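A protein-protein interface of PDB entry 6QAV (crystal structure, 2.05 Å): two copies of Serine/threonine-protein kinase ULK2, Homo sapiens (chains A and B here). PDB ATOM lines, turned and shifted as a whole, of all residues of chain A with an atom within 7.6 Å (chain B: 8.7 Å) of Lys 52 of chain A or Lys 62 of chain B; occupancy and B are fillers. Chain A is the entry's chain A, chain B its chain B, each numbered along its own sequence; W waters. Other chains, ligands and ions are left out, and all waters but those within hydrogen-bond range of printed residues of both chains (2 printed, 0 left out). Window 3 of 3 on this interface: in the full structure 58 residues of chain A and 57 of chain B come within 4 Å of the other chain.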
ATOM      1  N   PHE A  24     -42.081 -28.594  20.941  1.00  0.00           N
ATOM      2  CA  PHE A  24     -41.190 -29.725  20.988  1.00  0.00           C
ATOM      3  C   PHE A  24     -41.931 -31.057  20.741  1.00  0.00           C
ATOM      4  O   PHE A  24     -41.327 -32.130  20.907  1.00  0.00           O
ATOM      5  CB  PHE A  24     -40.422 -29.712  22.327  1.00  0.00           C
ATOM      6  CG  PHE A  24     -39.618 -28.451  22.550  1.00  0.00           C
ATOM      7  CD1 PHE A  24     -38.449 -28.232  21.832  1.00  0.00           C
ATOM      8  CD2 PHE A  24     -40.065 -27.456  23.396  1.00  0.00           C
ATOM      9  CE1 PHE A  24     -37.707 -27.077  21.998  1.00  0.00           C
ATOM     10  CE2 PHE A  24     -39.329 -26.284  23.565  1.00  0.00           C
ATOM     11  CZ  PHE A  24     -38.163 -26.093  22.832  1.00  0.00           C
ATOM     12  N   ASN A  46     -39.451 -34.149  20.495  1.00  0.00           N
ATOM     13  CA  ASN A  46     -38.134 -33.911  19.984  1.00  0.00           C
ATOM     14  C   ASN A  46     -37.174 -33.603  21.152  1.00  0.00           C
ATOM     15  O   ASN A  46     -37.010 -32.428  21.548  1.00  0.00           O
ATOM     16  CB  ASN A  46     -38.164 -32.792  18.942  1.00  0.00           C
ATOM     17  CG  ASN A  46     -36.850 -32.634  18.224  1.00  0.00           C
ATOM     18  OD1 ASN A  46     -35.807 -33.070  18.710  1.00  0.00           O
ATOM     19  ND2 ASN A  46     -36.866 -31.915  17.129  1.00  0.00           N
ATOM     20  N   LYS A  47     -36.540 -34.662  21.692  1.00  0.00           N
ATOM     21  CA  LYS A  47     -35.620 -34.561  22.840  1.00  0.00           C
ATOM     22  C   LYS A  47     -34.367 -33.750  22.486  1.00  0.00           C
ATOM     23  O   LYS A  47     -33.813 -33.039  23.338  1.00  0.00           O
ATOM     24  CB  LYS A  47     -35.176 -35.937  23.341  1.00  0.00           C
ATOM     25  CG  LYS A  47     -36.248 -36.781  24.009  1.00  0.00           C
ATOM     26  CD  LYS A  47     -35.699 -38.079  24.632  1.00  0.00           C
ATOM     27  CE  LYS A  47     -34.720 -38.797  23.735  1.00  0.00           C
ATOM     28  NZ  LYS A  47     -34.501 -40.216  24.126  1.00  0.00           N
ATOM     29  N   LYS A  48     -33.918 -33.852  21.236  1.00  0.00           N
ATOM     30  CA  LYS A  48     -32.715 -33.197  20.802  1.00  0.00           C
ATOM     31  C   LYS A  48     -32.905 -31.673  20.844  1.00  0.00           C
ATOM     32  O   LYS A  48     -32.051 -30.955  21.368  1.00  0.00           O
ATOM     33  CB  LYS A  48     -32.307 -33.640  19.398  1.00  0.00           C
ATOM     34  CG  LYS A  48     -30.933 -33.165  18.961  1.00  0.00           C
ATOM     35  CD  LYS A  48     -30.557 -33.593  17.555  1.00  0.00           C
ATOM     36  CE  LYS A  48     -29.140 -33.184  17.184  1.00  0.00           C
ATOM     37  NZ  LYS A  48     -28.394 -34.276  16.506  1.00  0.00           N
ATOM     38  N   ASN A  49     -33.993 -31.180  20.249  1.00  0.00           N
ATOM     39  CA  ASN A  49     -34.277 -29.753  20.224  1.00  0.00           C
ATOM     40  C   ASN A  49     -34.530 -29.253  21.640  1.00  0.00           C
ATOM     41  O   ASN A  49     -34.030 -28.209  22.027  1.00  0.00           O
ATOM     42  CB  ASN A  49     -35.458 -29.408  19.336  1.00  0.00           C
ATOM     43  CG  ASN A  49     -35.131 -28.310  18.356  1.00  0.00           C
ATOM     44  OD1 ASN A  49     -33.963 -28.003  18.123  1.00  0.00           O
ATOM     45  ND2 ASN A  49     -36.162 -27.746  17.744  1.00  0.00           N
ATOM     46  N   LEU A  50     -35.253 -30.043  22.435  1.00  0.00           N
ATOM     47  CA  LEU A  50     -35.525 -29.680  23.805  1.00  0.00           C
ATOM     48  C   LEU A  50     -34.202 -29.485  24.559  1.00  0.00           C
ATOM     49  O   LEU A  50     -34.069 -28.562  25.328  1.00  0.00           O
ATOM     50  CB  LEU A  50     -36.379 -30.804  24.406  1.00  0.00           C
ATOM     51  CG  LEU A  50     -37.278 -30.526  25.600  1.00  0.00           C
ATOM     52  CD1 LEU A  50     -37.887 -29.151  25.623  1.00  0.00           C
ATOM     53  CD2 LEU A  50     -38.416 -31.545  25.598  1.00  0.00           C
ATOM     54  N   SER A  51     -33.206 -30.368  24.313  1.00  0.00           N
ATOM     55  CA  SER A  51     -31.933 -30.310  25.029  1.00  0.00           C
ATOM     56  C   SER A  51     -31.177 -29.001  24.746  1.00  0.00           C
ATOM     57  O   SER A  51     -30.313 -28.611  25.510  1.00  0.00           O
ATOM     58  CB  SER A  51     -31.074 -31.497  24.712  1.00  0.00           C
ATOM     59  OG  SER A  51     -30.477 -31.333  23.446  1.00  0.00           O
ATOM     60  N   LYS A  52     -31.490 -28.331  23.641  1.00  0.00           N
ATOM     61  CA  LYS A  52     -30.867 -27.079  23.282  1.00  0.00           C
ATOM     62  C   LYS A  52     -31.644 -25.882  23.849  1.00  0.00           C
ATOM     63  O   LYS A  52     -31.263 -24.735  23.608  1.00  0.00           O
ATOM     64  CB  LYS A  52     -30.785 -26.950  21.768  1.00  0.00           C
ATOM     65  CG  LYS A  52     -29.890 -27.988  21.096  1.00  0.00           C
ATOM     66  CD  LYS A  52     -30.019 -27.891  19.599  1.00  0.00           C
ATOM     67  CE  LYS A  52     -28.981 -28.669  18.827  1.00  0.00           C
ATOM     68  NZ  LYS A  52     -28.714 -29.949  19.495  1.00  0.00           N
ATOM     69  N   SER A  53     -32.748 -26.137  24.542  1.00  0.00           N
ATOM     70  CA  SER A  53     -33.628 -25.060  24.967  1.00  0.00           C
ATOM     71  C   SER A  53     -33.613 -24.942  26.496  1.00  0.00           C
ATOM     72  O   SER A  53     -33.199 -25.874  27.206  1.00  0.00           O
ATOM     73  CB  SER A  53     -35.025 -25.246  24.450  1.00  0.00           C
ATOM     74  OG  SER A  53     -35.768 -25.970  25.373  1.00  0.00           O
ATOM     75  N   GLN A  54     -34.082 -23.800  26.997  1.00  0.00           N
ATOM     76  CA  GLN A  54     -34.146 -23.545  28.461  1.00  0.00           C
ATOM     77  C   GLN A  54     -35.341 -24.300  29.067  1.00  0.00           C
ATOM     78  O   GLN A  54     -35.440 -24.458  30.287  1.00  0.00           O
ATOM     79  CB  GLN A  54     -34.256 -22.047  28.760  1.00  0.00           C
ATOM     80  CG  GLN A  54     -33.086 -21.229  28.212  1.00  0.00           C
ATOM     81  CD  GLN A  54     -32.969 -19.849  28.818  1.00  0.00           C
ATOM     82  OE1 GLN A  54     -33.764 -19.460  29.668  1.00  0.00           O
ATOM     83  NE2 GLN A  54     -31.928 -19.123  28.424  1.00  0.00           N
ATOM     84  N   ILE A  55     -36.224 -24.811  28.210  1.00  0.00           N
ATOM     85  CA  ILE A  55     -37.435 -25.449  28.673  1.00  0.00           C
ATOM     86  C   ILE A  55     -37.145 -26.920  28.995  1.00  0.00           C
ATOM     87  O   ILE A  55     -36.537 -27.604  28.182  1.00  0.00           O
ATOM     88  CB  ILE A  55     -38.536 -25.265  27.612  1.00  0.00           C
ATOM     89  CG1 ILE A  55     -39.038 -23.803  27.628  1.00  0.00           C
ATOM     90  CG2 ILE A  55     -39.667 -26.255  27.860  1.00  0.00           C
ATOM     91  CD1 ILE A  55     -39.345 -23.222  26.285  1.00  0.00           C
ATOM     92  N   GLY B  58     -31.917 -32.025  34.010  1.00  0.00           N
ATOM     93  CA  GLY B  58     -31.577 -30.657  33.965  1.00  0.00           C
ATOM     94  C   GLY B  58     -30.966 -30.290  32.643  1.00  0.00           C
ATOM     95  O   GLY B  58     -31.219 -30.917  31.600  1.00  0.00           O
ATOM     96  N   LYS B  59     -30.125 -29.250  32.673  1.00  0.00           N
ATOM     97  CA  LYS B  59     -29.601 -28.586  31.483  1.00  0.00           C
ATOM     98  C   LYS B  59     -28.084 -28.394  31.618  1.00  0.00           C
ATOM     99  O   LYS B  59     -27.505 -27.447  31.048  1.00  0.00           O
ATOM    100  CB  LYS B  59     -30.294 -27.226  31.328  1.00  0.00           C
ATOM    101  CG  LYS B  59     -31.798 -27.298  31.120  1.00  0.00           C
ATOM    102  CD  LYS B  59     -32.151 -27.759  29.711  1.00  0.00           C
ATOM    103  CE  LYS B  59     -33.637 -27.904  29.529  1.00  0.00           C
ATOM    104  NZ  LYS B  59     -33.960 -28.416  28.185  1.00  0.00           N
ATOM    105  N   GLU B  60     -27.416 -29.315  32.320  1.00  0.00           N
ATOM    106  CA  GLU B  60     -25.972 -29.128  32.577  1.00  0.00           C
ATOM    107  C   GLU B  60     -25.197 -29.049  31.258  1.00  0.00           C
ATOM    108  O   GLU B  60     -24.313 -28.220  31.114  1.00  0.00           O
ATOM    109  CB  GLU B  60     -25.419 -30.192  33.512  1.00  0.00           C
ATOM    110  CG  GLU B  60     -23.912 -30.052  33.709  1.00  0.00           C
ATOM    111  CD  GLU B  60     -23.372 -30.848  34.869  1.00  0.00           C
ATOM    112  OE1 GLU B  60     -23.728 -32.046  34.970  1.00  0.00           O
ATOM    113  OE2 GLU B  60     -22.675 -30.235  35.695  1.00  0.00           O
ATOM    114  N   ILE B  61     -25.554 -29.889  30.290  1.00  0.00           N
ATOM    115  CA  ILE B  61     -24.825 -29.905  29.035  1.00  0.00           C
ATOM    116  C   ILE B  61     -24.992 -28.558  28.353  1.00  0.00           C
ATOM    117  O   ILE B  61     -24.012 -27.953  27.957  1.00  0.00           O
ATOM    118  CB  ILE B  61     -25.266 -31.068  28.133  1.00  0.00           C
ATOM    119  CG1 ILE B  61     -24.798 -32.409  28.683  1.00  0.00           C
ATOM    120  CG2 ILE B  61     -24.786 -30.875  26.711  1.00  0.00           C
ATOM    121  CD1 ILE B  61     -25.527 -33.605  28.071  1.00  0.00           C
ATOM    122  N   LYS B  62     -26.235 -28.104  28.199  1.00  0.00           N
ATOM    123  CA  LYS B  62     -26.495 -26.856  27.514  1.00  0.00           C
ATOM    124  C   LYS B  62     -25.770 -25.696  28.204  1.00  0.00           C
ATOM    125  O   LYS B  62     -25.201 -24.820  27.532  1.00  0.00           O
ATOM    126  CB  LYS B  62     -28.004 -26.613  27.471  1.00  0.00           C
ATOM    127  CG  LYS B  62     -28.416 -25.259  26.890  1.00  0.00           C
ATOM    128  CD  LYS B  62     -29.910 -25.011  27.035  1.00  0.00           C
ATOM    129  CE  LYS B  62     -30.314 -23.587  26.745  1.00  0.00           C
ATOM    130  NZ  LYS B  62     -29.964 -23.194  25.367  1.00  0.00           N
ATOM    131  N   ILE B  63     -25.863 -25.649  29.556  1.00  0.00           N
ATOM    132  CA  ILE B  63     -25.299 -24.550  30.314  1.00  0.00           C
ATOM    133  C   ILE B  63     -23.762 -24.526  30.125  1.00  0.00           C
ATOM    134  O   ILE B  63     -23.186 -23.476  29.863  1.00  0.00           O
ATOM    135  CB  ILE B  63     -25.677 -24.653  31.808  1.00  0.00           C
ATOM    136  CG1 ILE B  63     -27.150 -24.353  32.059  1.00  0.00           C
ATOM    137  CG2 ILE B  63     -24.790 -23.783  32.658  1.00  0.00           C
ATOM    138  CD1 ILE B  63     -27.662 -24.892  33.402  1.00  0.00           C
ATOM    139  N   LEU B  64     -23.104 -25.670  30.316  1.00  0.00           N
ATOM    140  CA  LEU B  64     -21.654 -25.710  30.246  1.00  0.00           C
ATOM    141  C   LEU B  64     -21.198 -25.509  28.797  1.00  0.00           C
ATOM    142  O   LEU B  64     -20.184 -24.861  28.590  1.00  0.00           O
ATOM    143  CB  LEU B  64     -21.149 -27.025  30.808  1.00  0.00           C
ATOM    144  CG  LEU B  64     -21.356 -27.189  32.310  1.00  0.00           C
ATOM    145  CD1 LEU B  64     -20.723 -28.472  32.791  1.00  0.00           C
ATOM    146  CD2 LEU B  64     -20.778 -25.993  33.077  1.00  0.00           C
ATOM    147  N   LYS B  65     -21.967 -26.026  27.818  1.00  0.00           N
ATOM    148  CA  LYS B  65     -21.650 -25.855  26.394  1.00  0.00           C
ATOM    149  C   LYS B  65     -21.614 -24.354  26.061  1.00  0.00           C
ATOM    150  O   LYS B  65     -20.694 -23.871  25.412  1.00  0.00           O
ATOM    151  CB  LYS B  65     -22.680 -26.604  25.539  1.00  0.00           C
ATOM    152  CG  LYS B  65     -22.485 -26.596  24.044  1.00  0.00           C
ATOM    153  CD  LYS B  65     -23.390 -27.607  23.341  1.00  0.00           C
ATOM    154  CE  LYS B  65     -22.803 -29.002  23.358  1.00  0.00           C
ATOM    155  NZ  LYS B  65     -23.667 -29.985  22.678  1.00  0.00           N
ATOM    156  N   GLU B  66     -22.592 -23.621  26.597  1.00  0.00           N
ATOM    157  CA  GLU B  66     -22.823 -22.251  26.209  1.00  0.00           C
ATOM    158  C   GLU B  66     -21.863 -21.315  26.963  1.00  0.00           C
ATOM    159  O   GLU B  66     -21.639 -20.231  26.478  1.00  0.00           O
ATOM    160  CB  GLU B  66     -24.317 -21.891  26.332  1.00  0.00           C
ATOM    161  CG  GLU B  66     -25.108 -22.413  25.136  1.00  0.00           C
ATOM    162  CD  GLU B  66     -26.625 -22.355  25.225  1.00  0.00           C
ATOM    163  OE1 GLU B  66     -27.140 -21.434  25.870  1.00  0.00           O
ATOM    164  OE2 GLU B  66     -27.290 -23.211  24.594  1.00  0.00           O
ATOM    165  N   LEU B  67     -21.321 -21.724  28.121  1.00  0.00           N
ATOM    166  CA  LEU B  67     -20.415 -20.862  28.877  1.00  0.00           C
ATOM    167  C   LEU B  67     -18.976 -21.087  28.439  1.00  0.00           C
ATOM    168  O   LEU B  67     -18.541 -22.235  28.222  1.00  0.00           O
ATOM    169  CB  LEU B  67     -20.555 -21.136  30.389  1.00  0.00           C
ATOM    170  CG  LEU B  67     -21.867 -20.624  30.983  1.00  0.00           C
ATOM    171  CD1 LEU B  67     -22.141 -21.228  32.328  1.00  0.00           C
ATOM    172  CD2 LEU B  67     -21.828 -19.113  31.116  1.00  0.00           C
ATOM    173  N   GLN B  68     -18.255 -19.982  28.336  1.00  0.00           N
ATOM    174  CA  GLN B  68     -16.828 -20.033  28.243  1.00  0.00           C
ATOM    175  C   GLN B  68     -16.285 -18.974  29.196  1.00  0.00           C
ATOM    176  O   GLN B  68     -16.250 -17.828  28.862  1.00  0.00           O
ATOM    177  CB  GLN B  68     -16.394 -19.853  26.782  1.00  0.00           C
ATOM    178  CG  GLN B  68     -14.902 -20.068  26.545  1.00  0.00           C
ATOM    179  CD  GLN B  68     -14.564 -21.383  25.853  1.00  0.00           C
ATOM    180  OE1 GLN B  68     -14.528 -21.473  24.617  1.00  0.00           O
ATOM    181  NE2 GLN B  68     -14.243 -22.416  26.643  1.00  0.00           N
ATOM    182  N   LEU B  75     -16.488 -27.540  29.356  1.00  0.00           N
ATOM    183  CA  LEU B  75     -16.967 -28.811  28.803  1.00  0.00           C
ATOM    184  C   LEU B  75     -16.244 -29.082  27.481  1.00  0.00           C
ATOM    185  O   LEU B  75     -16.328 -28.276  26.551  1.00  0.00           O
ATOM    186  CB  LEU B  75     -18.469 -28.707  28.542  1.00  0.00           C
ATOM    187  CG  LEU B  75     -19.115 -29.933  27.927  1.00  0.00           C
ATOM    188  CD1 LEU B  75     -19.011 -31.133  28.835  1.00  0.00           C
ATOM    189  CD2 LEU B  75     -20.550 -29.630  27.596  1.00  0.00           C
ATOM    190  N   VAL B  78     -19.112 -34.579  24.900  1.00  0.00           N
ATOM    191  CA  VAL B  78     -20.257 -35.305  25.396  1.00  0.00           C
ATOM    192  C   VAL B  78     -20.382 -36.620  24.636  1.00  0.00           C
ATOM    193  O   VAL B  78     -20.292 -36.601  23.432  1.00  0.00           O
ATOM    194  CB  VAL B  78     -21.557 -34.479  25.249  1.00  0.00           C
ATOM    195  CG1 VAL B  78     -22.804 -35.290  25.571  1.00  0.00           C
ATOM    196  CG2 VAL B  78     -21.509 -33.237  26.103  1.00  0.00           C
ATOM    197  N   LEU B  87     -20.009 -36.609  30.375  1.00  0.00           N
ATOM    198  CA  LEU B  87     -19.512 -35.278  30.129  1.00  0.00           C
ATOM    199  C   LEU B  87     -18.023 -35.290  30.430  1.00  0.00           C
ATOM    200  O   LEU B  87     -17.641 -35.691  31.536  1.00  0.00           O
ATOM    201  CB  LEU B  87     -20.225 -34.256  31.027  1.00  0.00           C
ATOM    202  CG  LEU B  87     -21.627 -33.825  30.628  1.00  0.00           C
ATOM    203  CD1 LEU B  87     -22.625 -34.959  30.733  1.00  0.00           C
ATOM    204  CD2 LEU B  87     -22.075 -32.630  31.462  1.00  0.00           C
ATOM    205  N   LYS B 129     -27.127 -14.654  32.111  1.00  0.00           N
ATOM    206  CA  LYS B 129     -27.768 -15.666  31.264  1.00  0.00           C
ATOM    207  C   LYS B 129     -29.070 -16.181  31.894  1.00  0.00           C
ATOM    208  O   LYS B 129     -29.722 -17.016  31.327  1.00  0.00           O
ATOM    209  CB  LYS B 129     -26.811 -16.825  31.012  1.00  0.00           C
ATOM    210  CG  LYS B 129     -25.502 -16.409  30.369  1.00  0.00           C
ATOM    211  CD  LYS B 129     -24.753 -17.499  29.741  1.00  0.00           C
ATOM    212  CE  LYS B 129     -24.759 -17.399  28.247  1.00  0.00           C
ATOM    213  NZ  LYS B 129     -23.673 -18.237  27.697  1.00  0.00           N
ATOM    214  N   ILE B 131     -29.386 -17.869  34.771  1.00  0.00           N
ATOM    215  CA  ILE B 131     -29.176 -19.192  35.345  1.00  0.00           C
ATOM    216  C   ILE B 131     -29.026 -19.041  36.838  1.00  0.00           C
ATOM    217  O   ILE B 131     -28.248 -18.207  37.278  1.00  0.00           O
ATOM    218  CB  ILE B 131     -27.918 -19.841  34.758  1.00  0.00           C
ATOM    219  CG1 ILE B 131     -28.050 -20.016  33.253  1.00  0.00           C
ATOM    220  CG2 ILE B 131     -27.544 -21.142  35.469  1.00  0.00           C
ATOM    221  CD1 ILE B 131     -26.727 -20.232  32.584  1.00  0.00           C
ATOM    222  N   PHE B 163     -23.883 -28.420  37.566  1.00  0.00           N
ATOM    223  CA  PHE B 163     -25.035 -27.644  37.212  1.00  0.00           C
ATOM    224  C   PHE B 163     -26.278 -28.532  37.002  1.00  0.00           C
ATOM    225  O   PHE B 163     -27.239 -28.111  36.330  1.00  0.00           O
ATOM    226  CB  PHE B 163     -24.702 -26.829  35.968  1.00  0.00           C
ATOM    227  CG  PHE B 163     -23.861 -25.622  36.272  1.00  0.00           C
ATOM    228  CD1 PHE B 163     -22.480 -25.731  36.385  1.00  0.00           C
ATOM    229  CD2 PHE B 163     -24.456 -24.381  36.469  1.00  0.00           C
ATOM    230  CE1 PHE B 163     -21.716 -24.629  36.721  1.00  0.00           C
ATOM    231  CE2 PHE B 163     -23.680 -23.285  36.784  1.00  0.00           C
ATOM    232  CZ  PHE B 163     -22.310 -23.424  36.894  1.00  0.00           C
ATOM    233  N   TYR B 168     -33.083 -22.216  34.459  1.00  0.00           N
ATOM    234  CA  TYR B 168     -33.167 -20.992  33.790  1.00  0.00           C
ATOM    235  C   TYR B 168     -34.370 -20.203  34.334  1.00  0.00           C
ATOM    236  O   TYR B 168     -35.473 -20.681  34.301  1.00  0.00           O
ATOM    237  CB  TYR B 168     -33.291 -21.234  32.287  1.00  0.00           C
ATOM    238  CG  TYR B 168     -32.023 -21.661  31.601  1.00  0.00           C
ATOM    239  CD1 TYR B 168     -31.058 -20.746  31.193  1.00  0.00           C
ATOM    240  CD2 TYR B 168     -31.779 -22.999  31.350  1.00  0.00           C
ATOM    241  CE1 TYR B 168     -29.924 -21.146  30.492  1.00  0.00           C
ATOM    242  CE2 TYR B 168     -30.644 -23.419  30.682  1.00  0.00           C
ATOM    243  CZ  TYR B 168     -29.722 -22.485  30.241  1.00  0.00           C
ATOM    244  OH  TYR B 168     -28.590 -22.876  29.565  1.00  0.00           O
ATOM    245  N   MET B 174     -40.703 -18.320  28.992  1.00  0.00           N
ATOM    246  CA  MET B 174     -40.416 -18.722  27.607  1.00  0.00           C
ATOM    247  C   MET B 174     -41.447 -19.752  27.131  1.00  0.00           C
ATOM    248  O   MET B 174     -41.911 -19.658  25.985  1.00  0.00           O
ATOM    249  CB  MET B 174     -39.011 -19.303  27.461  1.00  0.00           C
ATOM    250  CG  MET B 174     -37.940 -18.239  27.368  1.00  0.00           C
ATOM    251  SD  MET B 174     -36.299 -19.041  27.434  1.00  0.00           S
ATOM    252  CE  MET B 174     -35.247 -17.601  27.661  1.00  0.00           C
HETATM  253  O   HOH W   1     -28.875 -29.714  27.920  1.00  0.00           O
HETATM  254  O   HOH W   2     -35.044 -24.295  33.420  1.00  0.00           O
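Ser 51 of chain A touches Lys 62 of chain B.
Ser 53 of chain A touches Lys 62 of chain B.
Gln 54 of chain A touches Lys 59 of chain B.
N of Gln 54 of chain A touches CE of Lys 62 of chain B, at 3.8 Å.
CD1 of Tyr 168 of chain B touches CD of Gln 54 of chain A (3.2 Å).
Ser 51 of chain A touches just one residue of chain B: Lys 62 (3.6 Å).
Lys 52 of chain A touches one residue of chain B.
Of chain B, only Lys 59 (2.8 Å) and Lys 62 (3.4 Å) come within 4 Å of Ser 53 of chain A.
Printed residues of chain B within 4 Å of Gln 54 of chain A: Lys 59, Lys 62, Tyr 168 and Met 174.
Of the printed residues of chain B, Ile 55 of chain A touches Lys 59.
Ile 61 of chain B touches none of the printed residues of chain A.
Lys 62 of chain B touches four residues of chain A.
Printed residues of chain A within 4 Å of Tyr 168 of chain B: Gln 54.
The nearest residue of chain A that does not touch Lys 62 of chain B is Leu 50 of chain A (5.7 Å).
The nearest printed residue of chain B that does not touch Leu 50 of chain A is Lys 62 of chain B (5.7 Å).
O of Ser 53 of chain A sits at hydrogen-bond distance from NZ of Lys 59 of chain B.
The side-chain amino group of Lys 59 of chain B lies within hydrogen-bond range of the backbone carbonyl oxygen of Leu 50 of chain A (2.9 Å).
SD of Met 174 of chain B sits close to OE1 of Gln 54 of chain A (3.4 Å).
The backbone carbonyl oxygen (O) of Ile 55 of chain A is in hydrogen-bond range of the side-chain amino group (NZ) of Lys 59 of chain B (2.7 Å).
The backbone carbonyl oxygen of Lys 52 of chain A lies within hydrogen-bond range of the side-chain amino group of Lys 62 of chain B, 2.7 Å away.
NZ of Lys 62 of chain B is in salt-bridge range of OE2 of Glu 66 of chain B.
OG of Ser 53 of chain A lies within hydrogen-bond range of N of Ile 55 of chain A, 3.1 Å away.
O of Lys 48 of chain A is in hydrogen-bond range of OG of Ser 51 of chain A, at 2.6 Å.
The backbone carbonyl oxygen (O) of Leu 50 of chain A sits at hydrogen-bond distance from the side-chain hydroxyl (OG) of Ser 53 of chain A (3.1 Å).
Printed residues of chain B that touch a printed residue of chain A: Lys 59, Lys 62, Tyr 168 and Met 174.
Hydrophobic or aromatic side chains of chain B within 4 Å of the printed part of chain A: Tyr 168 and Met 174.
Along chain B the printed residues that touch a printed residue of chain A span positions 59 to 174.
Among the printed residues, no Asp or Glu carboxylate lies within 4 Å of a Lys or Arg side-chain nitrogen of the other chain.
Water W1 bridges O of Ser 51 of chain A (3.0 Å) and N of Lys 62 of chain B (3.1 Å).
Water W2 lies within hydrogen-bond range of the backbone NH of Tyr 168 of chain B (3.0 Å) and the backbone carbonyl oxygen of Gln 54 of chain A (3.2 Å).
No position is printed for both chains.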
